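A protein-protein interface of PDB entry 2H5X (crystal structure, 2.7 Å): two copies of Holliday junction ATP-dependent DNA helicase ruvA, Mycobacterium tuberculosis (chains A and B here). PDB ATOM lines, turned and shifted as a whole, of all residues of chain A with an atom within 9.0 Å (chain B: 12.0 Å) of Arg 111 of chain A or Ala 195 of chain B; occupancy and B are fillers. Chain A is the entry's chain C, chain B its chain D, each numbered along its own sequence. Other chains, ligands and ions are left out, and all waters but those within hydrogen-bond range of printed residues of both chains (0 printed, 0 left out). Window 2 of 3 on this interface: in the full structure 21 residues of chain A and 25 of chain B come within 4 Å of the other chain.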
ATOM      1  N   LEU A  84      20.551 -14.012   9.192  1.00  0.00           N
ATOM      2  CA  LEU A  84      20.254 -15.424   8.998  1.00  0.00           C
ATOM      3  C   LEU A  84      21.003 -15.993   7.795  1.00  0.00           C
ATOM      4  O   LEU A  84      21.531 -17.107   7.847  1.00  0.00           O
ATOM      5  CB  LEU A  84      18.747 -15.615   8.813  1.00  0.00           C
ATOM      6  CG  LEU A  84      18.251 -17.056   8.913  1.00  0.00           C
ATOM      7  CD1 LEU A  84      18.519 -17.571  10.316  1.00  0.00           C
ATOM      8  CD2 LEU A  84      16.769 -17.128   8.580  1.00  0.00           C
ATOM      9  N   ALA A  87      24.583 -16.401   8.662  1.00  0.00           N
ATOM     10  CA  ALA A  87      24.612 -17.506   9.617  1.00  0.00           C
ATOM     11  C   ALA A  87      24.585 -18.819   8.839  1.00  0.00           C
ATOM     12  O   ALA A  87      25.405 -19.708   9.067  1.00  0.00           O
ATOM     13  CB  ALA A  87      23.412 -17.429  10.555  1.00  0.00           C
ATOM     14  N   ALA A  88      23.636 -18.925   7.919  1.00  0.00           N
ATOM     15  CA  ALA A  88      23.498 -20.110   7.093  1.00  0.00           C
ATOM     16  C   ALA A  88      24.841 -20.438   6.430  1.00  0.00           C
ATOM     17  O   ALA A  88      25.348 -21.565   6.555  1.00  0.00           O
ATOM     18  CB  ALA A  88      22.434 -19.875   6.038  1.00  0.00           C
ATOM     19  N   ALA A  90      27.714 -19.450   7.250  1.00  0.00           N
ATOM     20  CA  ALA A  90      28.759 -19.682   8.224  1.00  0.00           C
ATOM     21  C   ALA A  90      28.694 -21.129   8.674  1.00  0.00           C
ATOM     22  O   ALA A  90      29.704 -21.702   9.090  1.00  0.00           O
ATOM     23  CB  ALA A  90      28.573 -18.766   9.408  1.00  0.00           C
ATOM     24  N   VAL A  91      27.502 -21.718   8.597  1.00  0.00           N
ATOM     25  CA  VAL A  91      27.320 -23.104   9.004  1.00  0.00           C
ATOM     26  C   VAL A  91      27.570 -24.053   7.840  1.00  0.00           C
ATOM     27  O   VAL A  91      27.964 -25.191   8.051  1.00  0.00           O
ATOM     28  CB  VAL A  91      25.898 -23.357   9.543  1.00  0.00           C
ATOM     29  CG1 VAL A  91      25.771 -24.795   9.995  1.00  0.00           C
ATOM     30  CG2 VAL A  91      25.592 -22.400  10.695  1.00  0.00           C
ATOM     31  N   HIS A  92      27.353 -23.572   6.620  1.00  0.00           N
ATOM     32  CA  HIS A  92      27.547 -24.375   5.414  1.00  0.00           C
ATOM     33  C   HIS A  92      28.143 -23.535   4.285  1.00  0.00           C
ATOM     34  O   HIS A  92      27.596 -22.496   3.910  1.00  0.00           O
ATOM     35  CB  HIS A  92      26.208 -24.950   4.934  1.00  0.00           C
ATOM     36  CG  HIS A  92      25.606 -25.955   5.867  1.00  0.00           C
ATOM     37  ND1 HIS A  92      24.246 -26.052   6.077  1.00  0.00           N
ATOM     38  CD2 HIS A  92      26.172 -26.918   6.631  1.00  0.00           C
ATOM     39  CE1 HIS A  92      24.000 -27.027   6.932  1.00  0.00           C
ATOM     40  NE2 HIS A  92      25.153 -27.570   7.284  1.00  0.00           N
ATOM     41  N   VAL A 100      22.579 -28.981   0.105  1.00  0.00           N
ATOM     42  CA  VAL A 100      21.491 -29.091   1.057  1.00  0.00           C
ATOM     43  C   VAL A 100      20.194 -28.615   0.415  1.00  0.00           C
ATOM     44  O   VAL A 100      19.134 -29.196   0.624  1.00  0.00           O
ATOM     45  CB  VAL A 100      21.749 -28.248   2.310  1.00  0.00           C
ATOM     46  CG1 VAL A 100      20.505 -28.238   3.192  1.00  0.00           C
ATOM     47  CG2 VAL A 100      22.929 -28.812   3.073  1.00  0.00           C
ATOM     48  N   ASN A 105      17.782 -31.345   1.764  1.00  0.00           N
ATOM     49  CA  ASN A 105      18.169 -31.976   3.030  1.00  0.00           C
ATOM     50  C   ASN A 105      17.746 -31.082   4.189  1.00  0.00           C
ATOM     51  O   ASN A 105      18.572 -30.421   4.811  1.00  0.00           O
ATOM     52  CB  ASN A 105      19.684 -32.198   3.094  1.00  0.00           C
ATOM     53  CG  ASN A 105      20.106 -32.978   4.330  1.00  0.00           C
ATOM     54  OD1 ASN A 105      19.506 -32.838   5.394  1.00  0.00           O
ATOM     55  ND2 ASN A 105      21.145 -33.796   4.196  1.00  0.00           N
ATOM     56  N   VAL A 106      16.452 -31.073   4.478  1.00  0.00           N
ATOM     57  CA  VAL A 106      15.909 -30.242   5.542  1.00  0.00           C
ATOM     58  C   VAL A 106      16.550 -30.470   6.918  1.00  0.00           C
ATOM     59  O   VAL A 106      16.608 -29.557   7.734  1.00  0.00           O
ATOM     60  CB  VAL A 106      14.375 -30.439   5.648  1.00  0.00           C
ATOM     61  CG1 VAL A 106      14.064 -31.844   6.140  1.00  0.00           C
ATOM     62  CG2 VAL A 106      13.770 -29.390   6.562  1.00  0.00           C
ATOM     63  N   ALA A 107      17.036 -31.681   7.168  1.00  0.00           N
ATOM     64  CA  ALA A 107      17.663 -32.006   8.452  1.00  0.00           C
ATOM     65  C   ALA A 107      18.956 -31.242   8.688  1.00  0.00           C
ATOM     66  O   ALA A 107      19.325 -30.973   9.832  1.00  0.00           O
ATOM     67  CB  ALA A 107      17.944 -33.491   8.527  1.00  0.00           C
ATOM     68  N   ALA A 108      19.654 -30.924   7.601  1.00  0.00           N
ATOM     69  CA  ALA A 108      20.918 -30.200   7.663  1.00  0.00           C
ATOM     70  C   ALA A 108      20.655 -28.704   7.722  1.00  0.00           C
ATOM     71  O   ALA A 108      21.357 -27.965   8.418  1.00  0.00           O
ATOM     72  CB  ALA A 108      21.761 -30.533   6.449  1.00  0.00           C
ATOM     73  N   LEU A 109      19.641 -28.260   6.980  1.00  0.00           N
ATOM     74  CA  LEU A 109      19.285 -26.851   6.967  1.00  0.00           C
ATOM     75  C   LEU A 109      18.903 -26.390   8.357  1.00  0.00           C
ATOM     76  O   LEU A 109      19.323 -25.331   8.814  1.00  0.00           O
ATOM     77  CB  LEU A 109      18.124 -26.596   6.015  1.00  0.00           C
ATOM     78  CG  LEU A 109      18.554 -26.066   4.655  1.00  0.00           C
ATOM     79  CD1 LEU A 109      17.342 -25.504   3.928  1.00  0.00           C
ATOM     80  CD2 LEU A 109      19.602 -24.982   4.852  1.00  0.00           C
ATOM     81  N   THR A 110      18.106 -27.203   9.035  1.00  0.00           N
ATOM     82  CA  THR A 110      17.669 -26.866  10.374  1.00  0.00           C
ATOM     83  C   THR A 110      18.836 -26.769  11.341  1.00  0.00           C
ATOM     84  O   THR A 110      18.674 -26.252  12.444  1.00  0.00           O
ATOM     85  CB  THR A 110      16.652 -27.880  10.898  1.00  0.00           C
ATOM     86  OG1 THR A 110      17.115 -29.205  10.608  1.00  0.00           O
ATOM     87  CG2 THR A 110      15.302 -27.658  10.243  1.00  0.00           C
ATOM     88  N   ARG A 111      20.009 -27.254  10.937  1.00  0.00           N
ATOM     89  CA  ARG A 111      21.188 -27.165  11.802  1.00  0.00           C
ATOM     90  C   ARG A 111      21.605 -25.705  11.937  1.00  0.00           C
ATOM     91  O   ARG A 111      22.316 -25.332  12.870  1.00  0.00           O
ATOM     92  CB  ARG A 111      22.357 -27.975  11.236  1.00  0.00           C
ATOM     93  CG  ARG A 111      22.237 -29.467  11.467  1.00  0.00           C
ATOM     94  CD  ARG A 111      23.177 -30.248  10.566  1.00  0.00           C
ATOM     95  NE  ARG A 111      22.784 -31.653  10.493  1.00  0.00           N
ATOM     96  CZ  ARG A 111      23.136 -32.485   9.517  1.00  0.00           C
ATOM     97  NH1 ARG A 111      23.902 -32.064   8.516  1.00  0.00           N
ATOM     98  NH2 ARG A 111      22.706 -33.740   9.541  1.00  0.00           N
ATOM     99  N   VAL A 112      21.161 -24.883  10.996  1.00  0.00           N
ATOM    100  CA  VAL A 112      21.465 -23.464  11.030  1.00  0.00           C
ATOM    101  C   VAL A 112      20.474 -22.801  11.986  1.00  0.00           C
ATOM    102  O   VAL A 112      19.256 -22.908  11.809  1.00  0.00           O
ATOM    103  CB  VAL A 112      21.333 -22.834   9.615  1.00  0.00           C
ATOM    104  CG1 VAL A 112      21.647 -21.351   9.669  1.00  0.00           C
ATOM    105  CG2 VAL A 112      22.259 -23.553   8.637  1.00  0.00           C
ATOM    106  N   PRO A 113      20.984 -22.128  13.027  1.00  0.00           N
ATOM    107  CA  PRO A 113      20.191 -21.427  14.044  1.00  0.00           C
ATOM    108  C   PRO A 113      19.313 -20.363  13.406  1.00  0.00           C
ATOM    109  O   PRO A 113      19.818 -19.487  12.700  1.00  0.00           O
ATOM    110  CB  PRO A 113      21.248 -20.793  14.944  1.00  0.00           C
ATOM    111  CG  PRO A 113      22.416 -21.694  14.796  1.00  0.00           C
ATOM    112  CD  PRO A 113      22.421 -22.015  13.325  1.00  0.00           C
ATOM    113  N   GLY A 114      18.010 -20.428  13.654  1.00  0.00           N
ATOM    114  CA  GLY A 114      17.111 -19.444  13.074  1.00  0.00           C
ATOM    115  C   GLY A 114      16.286 -19.998  11.926  1.00  0.00           C
ATOM    116  O   GLY A 114      15.328 -19.373  11.481  1.00  0.00           O
ATOM    117  N   ILE A 115      16.678 -21.172  11.440  1.00  0.00           N
ATOM    118  CA  ILE A 115      15.972 -21.846  10.362  1.00  0.00           C
ATOM    119  C   ILE A 115      15.411 -23.130  10.934  1.00  0.00           C
ATOM    120  O   ILE A 115      16.161 -24.058  11.256  1.00  0.00           O
ATOM    121  CB  ILE A 115      16.903 -22.254   9.222  1.00  0.00           C
ATOM    122  CG1 ILE A 115      17.599 -21.027   8.639  1.00  0.00           C
ATOM    123  CG2 ILE A 115      16.109 -23.015   8.170  1.00  0.00           C
ATOM    124  CD1 ILE A 115      18.645 -21.363   7.579  1.00  0.00           C
ATOM    125  N   GLY A 116      14.098 -23.202  11.060  1.00  0.00           N
ATOM    126  CA  GLY A 116      13.522 -24.413  11.598  1.00  0.00           C
ATOM    127  C   GLY A 116      12.721 -25.200  10.582  1.00  0.00           C
ATOM    128  O   GLY A 116      12.817 -24.974   9.373  1.00  0.00           O
ATOM    129  N   LYS A 117      11.954 -26.148  11.109  1.00  0.00           N
ATOM    130  CA  LYS A 117      11.044 -27.013  10.358  1.00  0.00           C
ATOM    131  C   LYS A 117      10.636 -26.520   8.956  1.00  0.00           C
ATOM    132  O   LYS A 117      11.277 -26.846   7.950  1.00  0.00           O
ATOM    133  CB  LYS A 117       9.781 -27.209  11.211  1.00  0.00           C
ATOM    134  CG  LYS A 117       9.487 -26.026  12.176  1.00  0.00           C
ATOM    135  CD  LYS A 117       9.508 -24.669  11.455  1.00  0.00           C
ATOM    136  CE  LYS A 117       9.534 -23.480  12.407  1.00  0.00           C
ATOM    137  NZ  LYS A 117       9.819 -22.207  11.677  1.00  0.00           N
ATOM    138  N   ALA A 120      12.924 -24.225   6.613  1.00  0.00           N
ATOM    139  CA  ALA A 120      13.812 -24.936   5.702  1.00  0.00           C
ATOM    140  C   ALA A 120      13.085 -25.391   4.442  1.00  0.00           C
ATOM    141  O   ALA A 120      13.601 -25.240   3.327  1.00  0.00           O
ATOM    142  CB  ALA A 120      14.424 -26.134   6.407  1.00  0.00           C
ATOM    143  N   MET A 123      12.549 -22.598   2.179  1.00  0.00           N
ATOM    144  CA  MET A 123      13.762 -22.328   1.414  1.00  0.00           C
ATOM    145  C   MET A 123      14.011 -23.380   0.338  1.00  0.00           C
ATOM    146  O   MET A 123      14.274 -23.040  -0.818  1.00  0.00           O
ATOM    147  CB  MET A 123      14.991 -22.252   2.333  1.00  0.00           C
ATOM    148  CG  MET A 123      15.179 -20.904   3.020  1.00  0.00           C
ATOM    149  SD  MET A 123      16.725 -20.758   3.935  1.00  0.00           S
ATOM    150  CE  MET A 123      16.260 -21.504   5.462  1.00  0.00           C
ATOM    151  N   LEU B 155      29.854 -17.571  18.381  1.00  0.00           N
ATOM    152  CA  LEU B 155      28.866 -18.603  18.092  1.00  0.00           C
ATOM    153  C   LEU B 155      27.469 -18.176  18.485  1.00  0.00           C
ATOM    154  O   LEU B 155      26.529 -18.288  17.699  1.00  0.00           O
ATOM    155  CB  LEU B 155      29.218 -19.884  18.825  1.00  0.00           C
ATOM    156  CG  LEU B 155      30.437 -20.595  18.267  1.00  0.00           C
ATOM    157  CD1 LEU B 155      30.773 -21.771  19.165  1.00  0.00           C
ATOM    158  CD2 LEU B 155      30.152 -21.061  16.851  1.00  0.00           C
ATOM    159  N   VAL B 156      27.321 -17.700  19.711  1.00  0.00           N
ATOM    160  CA  VAL B 156      26.025 -17.247  20.168  1.00  0.00           C
ATOM    161  C   VAL B 156      25.576 -16.114  19.243  1.00  0.00           C
ATOM    162  O   VAL B 156      24.380 -15.892  19.029  1.00  0.00           O
ATOM    163  CB  VAL B 156      26.109 -16.764  21.623  1.00  0.00           C
ATOM    164  CG1 VAL B 156      24.778 -16.157  22.057  1.00  0.00           C
ATOM    165  CG2 VAL B 156      26.473 -17.938  22.523  1.00  0.00           C
ATOM    166  N   GLY B 157      26.550 -15.409  18.678  1.00  0.00           N
ATOM    167  CA  GLY B 157      26.235 -14.325  17.768  1.00  0.00           C
ATOM    168  C   GLY B 157      25.600 -14.853  16.494  1.00  0.00           C
ATOM    169  O   GLY B 157      25.020 -14.095  15.713  1.00  0.00           O
ATOM    170  N   LEU B 158      25.715 -16.157  16.273  1.00  0.00           N
ATOM    171  CA  LEU B 158      25.136 -16.777  15.094  1.00  0.00           C
ATOM    172  C   LEU B 158      23.860 -17.506  15.488  1.00  0.00           C
ATOM    173  O   LEU B 158      23.349 -18.344  14.748  1.00  0.00           O
ATOM    174  CB  LEU B 158      26.132 -17.749  14.465  1.00  0.00           C
ATOM    175  CG  LEU B 158      27.444 -17.110  14.004  1.00  0.00           C
ATOM    176  CD1 LEU B 158      28.449 -18.197  13.680  1.00  0.00           C
ATOM    177  CD2 LEU B 158      27.193 -16.222  12.800  1.00  0.00           C
ATOM    178  N   GLY B 159      23.353 -17.190  16.671  1.00  0.00           N
ATOM    179  CA  GLY B 159      22.126 -17.813  17.119  1.00  0.00           C
ATOM    180  C   GLY B 159      22.260 -19.096  17.908  1.00  0.00           C
ATOM    181  O   GLY B 159      21.278 -19.560  18.483  1.00  0.00           O
ATOM    182  N   PHE B 160      23.447 -19.685  17.954  1.00  0.00           N
ATOM    183  CA  PHE B 160      23.617 -20.926  18.706  1.00  0.00           C
ATOM    184  C   PHE B 160      23.399 -20.710  20.202  1.00  0.00           C
ATOM    185  O   PHE B 160      23.648 -19.620  20.724  1.00  0.00           O
ATOM    186  CB  PHE B 160      25.013 -21.508  18.481  1.00  0.00           C
ATOM    187  CG  PHE B 160      25.193 -22.174  17.144  1.00  0.00           C
ATOM    188  CD1 PHE B 160      24.749 -23.482  16.946  1.00  0.00           C
ATOM    189  CD2 PHE B 160      25.841 -21.508  16.097  1.00  0.00           C
ATOM    190  CE1 PHE B 160      24.946 -24.128  15.738  1.00  0.00           C
ATOM    191  CE2 PHE B 160      26.048 -22.142  14.876  1.00  0.00           C
ATOM    192  CZ  PHE B 160      25.599 -23.461  14.693  1.00  0.00           C
ATOM    193  N   ALA B 161      22.932 -21.749  20.888  1.00  0.00           N
ATOM    194  CA  ALA B 161      22.692 -21.669  22.324  1.00  0.00           C
ATOM    195  C   ALA B 161      24.009 -21.814  23.084  1.00  0.00           C
ATOM    196  O   ALA B 161      24.782 -22.742  22.839  1.00  0.00           O
ATOM    197  CB  ALA B 161      21.718 -22.760  22.756  1.00  0.00           C
ATOM    198  N   GLN B 164      25.295 -25.233  24.072  1.00  0.00           N
ATOM    199  CA  GLN B 164      25.754 -25.994  22.912  1.00  0.00           C
ATOM    200  C   GLN B 164      27.007 -25.355  22.322  1.00  0.00           C
ATOM    201  O   GLN B 164      27.872 -26.042  21.775  1.00  0.00           O
ATOM    202  CB  GLN B 164      24.649 -26.044  21.859  1.00  0.00           C
ATOM    203  CG  GLN B 164      24.956 -26.924  20.666  1.00  0.00           C
ATOM    204  CD  GLN B 164      23.905 -26.806  19.577  1.00  0.00           C
ATOM    205  OE1 GLN B 164      23.971 -27.494  18.556  1.00  0.00           O
ATOM    206  NE2 GLN B 164      22.929 -25.924  19.787  1.00  0.00           N
ATOM    207  N   ALA B 165      27.086 -24.033  22.434  1.00  0.00           N
ATOM    208  CA  ALA B 165      28.230 -23.284  21.934  1.00  0.00           C
ATOM    209  C   ALA B 165      29.466 -23.664  22.745  1.00  0.00           C
ATOM    210  O   ALA B 165      30.528 -23.941  22.186  1.00  0.00           O
ATOM    211  CB  ALA B 165      27.963 -21.792  22.051  1.00  0.00           C
ATOM    212  N   ALA B 168      31.044 -27.243  22.360  1.00  0.00           N
ATOM    213  CA  ALA B 168      31.689 -27.572  21.100  1.00  0.00           C
ATOM    214  C   ALA B 168      33.043 -26.890  21.108  1.00  0.00           C
ATOM    215  O   ALA B 168      33.994 -27.350  20.469  1.00  0.00           O
ATOM    216  CB  ALA B 168      30.837 -27.082  19.923  1.00  0.00           C
ATOM    217  N   SER B 187      36.426 -24.209  13.353  1.00  0.00           N
ATOM    218  CA  SER B 187      36.536 -25.611  13.696  1.00  0.00           C
ATOM    219  C   SER B 187      35.273 -26.037  14.433  1.00  0.00           C
ATOM    220  O   SER B 187      34.721 -27.113  14.168  1.00  0.00           O
ATOM    221  CB  SER B 187      37.769 -25.833  14.565  1.00  0.00           C
ATOM    222  OG  SER B 187      37.973 -27.209  14.807  1.00  0.00           O
ATOM    223  N   ALA B 188      34.806 -25.186  15.345  1.00  0.00           N
ATOM    224  CA  ALA B 188      33.595 -25.478  16.112  1.00  0.00           C
ATOM    225  C   ALA B 188      32.358 -25.458  15.214  1.00  0.00           C
ATOM    226  O   ALA B 188      31.364 -26.130  15.493  1.00  0.00           O
ATOM    227  CB  ALA B 188      33.430 -24.465  17.246  1.00  0.00           C
ATOM    228  N   LEU B 189      32.427 -24.680  14.136  1.00  0.00           N
ATOM    229  CA  LEU B 189      31.309 -24.586  13.204  1.00  0.00           C
ATOM    230  C   LEU B 189      31.128 -25.875  12.424  1.00  0.00           C
ATOM    231  O   LEU B 189      30.010 -26.370  12.306  1.00  0.00           O
ATOM    232  CB  LEU B 189      31.499 -23.399  12.260  1.00  0.00           C
ATOM    233  CG  LEU B 189      31.170 -22.097  12.996  1.00  0.00           C
ATOM    234  CD1 LEU B 189      31.425 -20.896  12.109  1.00  0.00           C
ATOM    235  CD2 LEU B 189      29.710 -22.137  13.452  1.00  0.00           C
ATOM    236  N   SER B 190      32.222 -26.429  11.906  1.00  0.00           N
ATOM    237  CA  SER B 190      32.121 -27.680  11.163  1.00  0.00           C
ATOM    238  C   SER B 190      31.485 -28.728  12.083  1.00  0.00           C
ATOM    239  O   SER B 190      30.681 -29.552  11.649  1.00  0.00           O
ATOM    240  CB  SER B 190      33.499 -28.161  10.708  1.00  0.00           C
ATOM    241  OG  SER B 190      34.238 -28.657  11.799  1.00  0.00           O
ATOM    242  N   LEU B 191      31.836 -28.673  13.362  1.00  0.00           N
ATOM    243  CA  LEU B 191      31.305 -29.604  14.345  1.00  0.00           C
ATOM    244  C   LEU B 191      29.819 -29.379  14.553  1.00  0.00           C
ATOM    245  O   LEU B 191      29.085 -30.309  14.877  1.00  0.00           O
ATOM    246  CB  LEU B 191      32.033 -29.423  15.677  1.00  0.00           C
ATOM    247  CG  LEU B 191      32.770 -30.625  16.268  1.00  0.00           C
ATOM    248  CD1 LEU B 191      33.677 -31.263  15.222  1.00  0.00           C
ATOM    249  CD2 LEU B 191      33.578 -30.156  17.468  1.00  0.00           C
ATOM    250  N   LEU B 192      29.378 -28.138  14.374  1.00  0.00           N
ATOM    251  CA  LEU B 192      27.972 -27.819  14.568  1.00  0.00           C
ATOM    252  C   LEU B 192      27.132 -28.065  13.304  1.00  0.00           C
ATOM    253  O   LEU B 192      25.910 -28.226  13.377  1.00  0.00           O
ATOM    254  CB  LEU B 192      27.830 -26.376  15.070  1.00  0.00           C
ATOM    255  CG  LEU B 192      28.360 -26.132  16.490  1.00  0.00           C
ATOM    256  CD1 LEU B 192      28.330 -24.648  16.822  1.00  0.00           C
ATOM    257  CD2 LEU B 192      27.520 -26.913  17.478  1.00  0.00           C
ATOM    258  N   GLY B 193      27.794 -28.100  12.151  1.00  0.00           N
ATOM    259  CA  GLY B 193      27.093 -28.379  10.911  1.00  0.00           C
ATOM    260  C   GLY B 193      27.104 -29.890  10.758  1.00  0.00           C
ATOM    261  O   GLY B 193      26.749 -30.449   9.715  1.00  0.00           O
ATOM    262  N   LYS B 194      27.530 -30.535  11.841  1.00  0.00           N
ATOM    263  CA  LYS B 194      27.656 -31.982  11.975  1.00  0.00           C
ATOM    264  C   LYS B 194      26.471 -32.779  11.452  1.00  0.00           C
ATOM    265  O   LYS B 194      25.893 -32.466  10.416  1.00  0.00           O
ATOM    266  CB  LYS B 194      27.864 -32.332  13.453  1.00  0.00           C
ATOM    267  CG  LYS B 194      26.580 -32.275  14.316  1.00  0.00           C
ATOM    268  CD  LYS B 194      25.780 -30.991  14.111  1.00  0.00           C
ATOM    269  CE  LYS B 194      24.393 -31.076  14.735  1.00  0.00           C
ATOM    270  NZ  LYS B 194      24.426 -31.250  16.211  1.00  0.00           N
ATOM    271  N   ALA B 195      26.140 -33.842  12.184  1.00  0.00           N
ATOM    272  CA  ALA B 195      25.030 -34.727  11.863  1.00  0.00           C
ATOM    273  C   ALA B 195      24.629 -35.489  13.128  1.00  0.00           C
ATOM    274  O   ALA B 195      23.471 -35.342  13.566  1.00  0.00           O
ATOM    275  CB  ALA B 195      25.443 -35.706  10.773  1.00  0.00           C
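No position is printed for both chains. Of the 8 pairs that touch across the chains among the printed residues, none has its exchanged pair printed and touching as well.
Hydrophobic or aromatic side chains of chain A within 4 Å of the printed part of chain B: Val 91 and Pro 113. Hydrophobic or aromatic side chains of chain B that line the printed part of chain A: Phe 160, Leu 189 and Ala 195. Among the printed residues, 8 pairs touch across the chains. Among the printed residues, no Asp or Glu carboxylate lies within 4 Å of a Lys or Arg side-chain nitrogen of the other chain.
Ala 88 of chain A touches none of the printed residues of chain B. Val 91 of chain A touches just one residue of chain B: Gly 193 (3.9 Å). No residue of chain B comes within 4 Å of Ala 107 of chain A. No residue of chain B comes within 4 Å of Ala 108 of chain A. No residue of chain B comes within 4 Å of Val 112 of chain A. No residue of chain B comes within 4 Å of Ile 115 of chain A. Gly 116 of chain A touches none of the printed residues of chain B. Printed residues of chain A within 4 Å of Gly 159 of chain B: Pro 113. Of the printed residues of chain A, Phe 160 of chain B touches Pro 113 (3.6 Å). Of the printed residues of chain A, Gly 193 of chain B touches Val 91 (3.9 Å) and Arg 111 (3.5 Å). Printed residues of chain A within 4 Å of Ala 195 of chain B: Arg 111. The nearest residue of chain B that does not touch Arg 111 of chain A is Phe 160 of chain B (4.1 Å).
Among the printed residues, pairs that only touch across the chains: Pro 113 of chain A with Leu 158 of chain B (3.2 Å), Arg 111 of chain A with Ala 195 of chain B (3.4 Å), Pro 113 of chain A with Gly 159 of chain B (3.6 Å), Ala 90 of chain A with Leu 189 of chain B (3.6 Å), Pro 113 of chain A with Phe 160 of chain B (3.6 Å) and Val 91 of chain A with Gly 193 of chain B (3.9 Å).
N of Phe 160 of chain B sits at hydrogen-bond distance from O of Leu 155 of chain B.
The backbone carbonyl oxygen (O) of Gly 193 of chain B lies within hydrogen-bond range of the guanidinium group (NH1) of Arg 111 of chain A. The guanidinium group of Arg 111 of chain A sits at hydrogen-bond distance from the backbone carbonyl oxygen of Lys 194 of chain B, 2.8 Å away.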
